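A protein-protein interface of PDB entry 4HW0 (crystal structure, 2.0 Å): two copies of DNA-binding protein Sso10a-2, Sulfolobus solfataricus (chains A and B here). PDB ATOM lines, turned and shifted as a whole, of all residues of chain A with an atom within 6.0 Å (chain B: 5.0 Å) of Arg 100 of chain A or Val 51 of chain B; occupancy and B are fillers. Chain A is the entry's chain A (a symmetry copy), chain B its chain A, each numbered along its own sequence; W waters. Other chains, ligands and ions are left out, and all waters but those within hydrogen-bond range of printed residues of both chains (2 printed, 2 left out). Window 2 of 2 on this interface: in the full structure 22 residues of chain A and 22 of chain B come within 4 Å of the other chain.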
ATOM      1  N   GLU A  93      -4.530  35.989  28.791  1.00  0.00           N
ATOM      2  CA  GLU A  93      -3.893  36.230  27.483  1.00  0.00           C
ATOM      3  C   GLU A  93      -2.625  35.411  27.349  1.00  0.00           C
ATOM      4  O   GLU A  93      -2.324  34.908  26.285  1.00  0.00           O
ATOM      5  CB  GLU A  93      -3.535  37.726  27.261  1.00  0.00           C
ATOM      6  CG  GLU A  93      -4.712  38.682  27.075  1.00  0.00           C
ATOM      7  CD  GLU A  93      -4.321  40.192  27.214  1.00  0.00           C
ATOM      8  OE1 GLU A  93      -3.102  40.550  27.317  1.00  0.00           O
ATOM      9  OE2 GLU A  93      -5.253  41.039  27.265  1.00  0.00           O
ATOM     10  N   SER A  96      -3.617  31.948  26.493  1.00  0.00           N
ATOM     11  CA  SER A  96      -4.125  31.914  25.131  1.00  0.00           C
ATOM     12  C   SER A  96      -2.990  31.896  24.070  1.00  0.00           C
ATOM     13  O   SER A  96      -3.077  31.227  23.038  1.00  0.00           O
ATOM     14  CB  SER A  96      -5.178  33.054  24.941  1.00  0.00           C
ATOM     15  OG  SER A  96      -5.778  32.957  23.656  1.00  0.00           O
ATOM     16  N   GLU A  97      -1.941  32.698  24.294  1.00  0.00           N
ATOM     17  CA  GLU A  97      -0.791  32.712  23.413  1.00  0.00           C
ATOM     18  C   GLU A  97      -0.210  31.350  23.184  1.00  0.00           C
ATOM     19  O   GLU A  97       0.385  31.096  22.147  1.00  0.00           O
ATOM     20  CB  GLU A  97       0.343  33.603  23.981  1.00  0.00           C
ATOM     21  CG  GLU A  97       0.163  35.114  23.917  1.00  0.00           C
ATOM     22  CD  GLU A  97       1.217  35.873  24.813  1.00  0.00           C
ATOM     23  OE1 GLU A  97       2.307  35.298  25.236  1.00  0.00           O
ATOM     24  OE2 GLU A  97       0.929  37.058  25.129  1.00  0.00           O
ATOM     25  N   LEU A  98      -0.284  30.472  24.191  1.00  0.00           N
ATOM     26  CA  LEU A  98       0.256  29.136  24.074  1.00  0.00           C
ATOM     27  C   LEU A  98      -0.714  28.142  23.420  1.00  0.00           C
ATOM     28  O   LEU A  98      -0.349  27.012  23.168  1.00  0.00           O
ATOM     29  CB  LEU A  98       0.669  28.602  25.454  1.00  0.00           C
ATOM     30  CG  LEU A  98       1.935  29.248  26.001  1.00  0.00           C
ATOM     31  CD1 LEU A  98       2.063  29.083  27.482  1.00  0.00           C
ATOM     32  CD2 LEU A  98       3.111  28.588  25.368  1.00  0.00           C
ATOM     33  N   LEU A  99      -1.938  28.577  23.170  1.00  0.00           N
ATOM     34  CA  LEU A  99      -2.958  27.704  22.554  1.00  0.00           C
ATOM     35  C   LEU A  99      -3.167  27.923  21.030  1.00  0.00           C
ATOM     36  O   LEU A  99      -4.253  27.897  20.544  1.00  0.00           O
ATOM     37  CB  LEU A  99      -4.243  27.932  23.338  1.00  0.00           C
ATOM     38  CG  LEU A  99      -4.147  27.425  24.793  1.00  0.00           C
ATOM     39  CD1 LEU A  99      -5.490  27.726  25.459  1.00  0.00           C
ATOM     40  CD2 LEU A  99      -3.787  25.964  24.790  1.00  0.00           C
ATOM     41  N   ARG A 100      -2.061  28.068  20.322  1.00  0.00           N
ATOM     42  CA  ARG A 100      -2.045  28.272  18.881  1.00  0.00           C
ATOM     43  C   ARG A 100      -1.267  27.211  18.324  1.00  0.00           C
ATOM     44  O   ARG A 100      -0.553  26.514  19.020  1.00  0.00           O
ATOM     45  CB  ARG A 100      -1.508  29.642  18.448  1.00  0.00           C
ATOM     46  CG  ARG A 100      -2.509  30.724  18.800  1.00  0.00           C
ATOM     47  CD  ARG A 100      -2.067  32.147  18.663  1.00  0.00           C
ATOM     48  NE  ARG A 100      -3.182  33.116  18.629  1.00  0.00           N
ATOM     49  CZ  ARG A 100      -3.947  33.506  19.648  1.00  0.00           C
ATOM     50  NH1 ARG A 100      -3.781  33.008  20.860  1.00  0.00           N
ATOM     51  NH2 ARG A 100      -4.935  34.404  19.463  1.00  0.00           N
ATOM     52  N   THR A 101      -1.469  27.018  17.040  1.00  0.00           N
ATOM     53  CA  THR A 101      -0.647  26.144  16.261  1.00  0.00           C
ATOM     54  C   THR A 101      -0.753  26.539  14.801  1.00  0.00           C
ATOM     55  O   THR A 101      -1.837  26.930  14.372  1.00  0.00           O
ATOM     56  CB  THR A 101      -1.158  24.723  16.310  1.00  0.00           C
ATOM     57  OG1 THR A 101      -0.303  23.957  15.479  1.00  0.00           O
ATOM     58  CG2 THR A 101      -2.640  24.601  15.800  1.00  0.00           C
ATOM     59  N   ASP A 102       0.359  26.408  14.064  1.00  0.00           N
ATOM     60  CA  ASP A 102       0.408  26.521  12.538  1.00  0.00           C
ATOM     61  C   ASP A 102       0.660  25.171  11.784  1.00  0.00           C
ATOM     62  O   ASP A 102       0.868  25.159  10.553  1.00  0.00           O
ATOM     63  CB  ASP A 102       1.414  27.618  12.064  1.00  0.00           C
ATOM     64  CG  ASP A 102       2.774  27.568  12.831  1.00  0.00           C
ATOM     65  OD1 ASP A 102       3.405  26.461  12.821  1.00  0.00           O
ATOM     66  OD2 ASP A 102       3.167  28.610  13.473  1.00  0.00           O
ATOM     67  N   GLN B  47      -6.442  18.123  21.614  1.00  0.00           N
ATOM     68  CA  GLN B  47      -6.175  19.534  21.650  1.00  0.00           C
ATOM     69  C   GLN B  47      -4.766  19.891  22.138  1.00  0.00           C
ATOM     70  O   GLN B  47      -4.067  20.693  21.507  1.00  0.00           O
ATOM     71  CB  GLN B  47      -7.215  20.278  22.423  1.00  0.00           C
ATOM     72  CG  GLN B  47      -8.598  20.238  21.741  1.00  0.00           C
ATOM     73  CD  GLN B  47      -9.524  21.222  22.376  1.00  0.00           C
ATOM     74  OE1 GLN B  47      -9.329  21.588  23.561  1.00  0.00           O
ATOM     75  NE2 GLN B  47     -10.612  21.564  21.687  1.00  0.00           N
ATOM     76  N   LEU B  48      -4.333  19.257  23.203  1.00  0.00           N
ATOM     77  CA  LEU B  48      -2.992  19.503  23.768  1.00  0.00           C
ATOM     78  C   LEU B  48      -1.897  19.050  22.841  1.00  0.00           C
ATOM     79  O   LEU B  48      -0.836  19.696  22.750  1.00  0.00           O
ATOM     80  CB  LEU B  48      -2.893  18.777  25.138  1.00  0.00           C
ATOM     81  CG  LEU B  48      -3.688  19.479  26.213  1.00  0.00           C
ATOM     82  CD1 LEU B  48      -3.795  18.694  27.510  1.00  0.00           C
ATOM     83  CD2 LEU B  48      -3.139  20.878  26.532  1.00  0.00           C
ATOM     84  N   VAL B  49      -2.105  17.935  22.143  1.00  0.00           N
ATOM     85  CA  VAL B  49      -1.132  17.519  21.071  1.00  0.00           C
ATOM     86  C   VAL B  49      -1.132  18.534  19.961  1.00  0.00           C
ATOM     87  O   VAL B  49      -0.044  19.001  19.508  1.00  0.00           O
ATOM     88  CB  VAL B  49      -1.454  16.100  20.535  1.00  0.00           C
ATOM     89  CG1 VAL B  49      -0.581  15.762  19.352  1.00  0.00           C
ATOM     90  CG2 VAL B  49      -1.325  15.028  21.657  1.00  0.00           C
ATOM     91  N   LYS B  50      -2.313  18.984  19.572  1.00  0.00           N
ATOM     92  CA  LYS B  50      -2.404  19.965  18.471  1.00  0.00           C
ATOM     93  C   LYS B  50      -1.718  21.246  18.784  1.00  0.00           C
ATOM     94  O   LYS B  50      -1.073  21.835  17.887  1.00  0.00           O
ATOM     95  CB  LYS B  50      -3.839  20.293  18.162  1.00  0.00           C
ATOM     96  CG  LYS B  50      -4.648  19.186  17.524  1.00  0.00           C
ATOM     97  CD  LYS B  50      -4.090  18.787  16.198  1.00  0.00           C
ATOM     98  CE  LYS B  50      -5.197  18.113  15.391  1.00  0.00           C
ATOM     99  NZ  LYS B  50      -5.288  16.651  15.678  1.00  0.00           N
ATOM    100  N   VAL B  51      -1.856  21.765  19.989  1.00  0.00           N
ATOM    101  CA  VAL B  51      -1.185  23.033  20.303  1.00  0.00           C
ATOM    102  C   VAL B  51       0.277  22.842  20.776  1.00  0.00           C
ATOM    103  O   VAL B  51       0.866  23.764  21.247  1.00  0.00           O
ATOM    104  CB  VAL B  51      -1.954  23.847  21.335  1.00  0.00           C
ATOM    105  CG1 VAL B  51      -3.342  24.111  20.837  1.00  0.00           C
ATOM    106  CG2 VAL B  51      -2.026  23.110  22.715  1.00  0.00           C
ATOM    107  N   GLY B  52       0.797  21.620  20.737  1.00  0.00           N
ATOM    108  CA  GLY B  52       2.213  21.370  21.005  1.00  0.00           C
ATOM    109  C   GLY B  52       2.568  21.271  22.497  1.00  0.00           C
ATOM    110  O   GLY B  52       3.744  21.359  22.858  1.00  0.00           O
ATOM    111  N   ALA B  53       1.576  21.039  23.325  1.00  0.00           N
ATOM    112  CA  ALA B  53       1.792  20.900  24.799  1.00  0.00           C
ATOM    113  C   ALA B  53       2.159  19.481  25.200  1.00  0.00           C
ATOM    114  O   ALA B  53       2.853  19.263  26.178  1.00  0.00           O
ATOM    115  CB  ALA B  53       0.569  21.356  25.547  1.00  0.00           C
ATOM    116  N   LYS B  70       6.939  23.538  25.796  1.00  0.00           N
ATOM    117  CA  LYS B  70       5.803  24.466  25.636  1.00  0.00           C
ATOM    118  C   LYS B  70       4.648  24.119  26.588  1.00  0.00           C
ATOM    119  O   LYS B  70       4.014  24.958  27.177  1.00  0.00           O
ATOM    120  CB  LYS B  70       5.336  24.445  24.187  1.00  0.00           C
ATOM    121  CG  LYS B  70       4.241  25.432  23.897  1.00  0.00           C
ATOM    122  CD  LYS B  70       3.835  25.442  22.399  1.00  0.00           C
ATOM    123  CE  LYS B  70       2.724  26.427  22.257  1.00  0.00           C
ATOM    124  NZ  LYS B  70       2.040  26.256  20.948  1.00  0.00           N
ATOM    125  N   LEU B  74       2.717  26.137  29.469  1.00  0.00           N
ATOM    126  CA  LEU B  74       1.263  26.224  29.524  1.00  0.00           C
ATOM    127  C   LEU B  74       0.733  25.863  30.908  1.00  0.00           C
ATOM    128  O   LEU B  74      -0.107  26.557  31.459  1.00  0.00           O
ATOM    129  CB  LEU B  74       0.662  25.344  28.441  1.00  0.00           C
ATOM    130  CG  LEU B  74      -0.861  25.313  28.352  1.00  0.00           C
ATOM    131  CD1 LEU B  74      -1.461  26.680  28.104  1.00  0.00           C
ATOM    132  CD2 LEU B  74      -1.301  24.281  27.295  1.00  0.00           C
HETATM  133  O   HOH W   1       0.871  28.900  20.742  1.00  0.00           O
HETATM  134  O   HOH W   2       0.696  24.436  24.116  1.00  0.00           O
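The side-chain amino group (NZ) of Lys 70 of chain B is in hydrogen-bond range of the backbone carbonyl oxygen (O) of Arg 100 of chain A. The side-chain hydroxyl (OG1) of Thr 101 of chain A lies close to the backbone carbonyl oxygen (O) of Lys 50 of chain B, at 3.3 Å. O of Leu 98 of chain A sits close to NZ of Lys 70 of chain B (3.3 Å).
O of Val 51 of chain B is in hydrogen-bond range of NZ of Lys 70 of chain B (2.8 Å). The backbone carbonyl oxygen (O) of Ser 96 of chain A lies within hydrogen-bond range of the guanidinium group (NH1) of Arg 100 of chain A (2.9 Å).
Among the printed residues, pairs that only touch across the chains: Leu 98 of chain A with Leu 74 of chain B, Arg 100 of chain A with Val 51 of chain B, Leu 99 of chain A with Val 51 of chain B, Leu 99 of chain A with Leu 74 of chain B and Leu 98 of chain A with Val 51 of chain B.
Printed residues of chain B within 4 Å of Arg 100 of chain A: Val 51 and Lys 70. Val 49 of chain B touches none of the printed residues of chain A. Of the printed residues of chain A, Lys 50 of chain B touches Thr 101. Of chain A, only Leu 98, Leu 99 and Arg 100 come within 4 Å of Val 51 of chain B. Of the printed residues of chain A, Lys 70 of chain B touches Leu 98 and Arg 100.
Hydrophobic or aromatic side chains of chain B that line the printed part of chain A: Val 51 and Leu 74. Hydrophobic or aromatic side chains of chain A within 4 Å of the printed part of chain B: Leu 98 and Leu 99. Among the printed residues, no Asp or Glu carboxylate lies within 4 Å of a Lys or Arg side-chain nitrogen of the other chain.
No position is printed for both chains.
Water W1 lies within hydrogen-bond range of O of Glu 97 of chain A (2.7 Å), NZ of Lys 70 of chain B (2.9 Å), N of Arg 100 of chain A (3.1 Å) and O of Leu 98 of chain A (3.3 Å). Water W2 lies within hydrogen-bond range of O of Leu 98 of chain A (2.9 Å) and O of Val 51 of chain B (3.0 Å).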
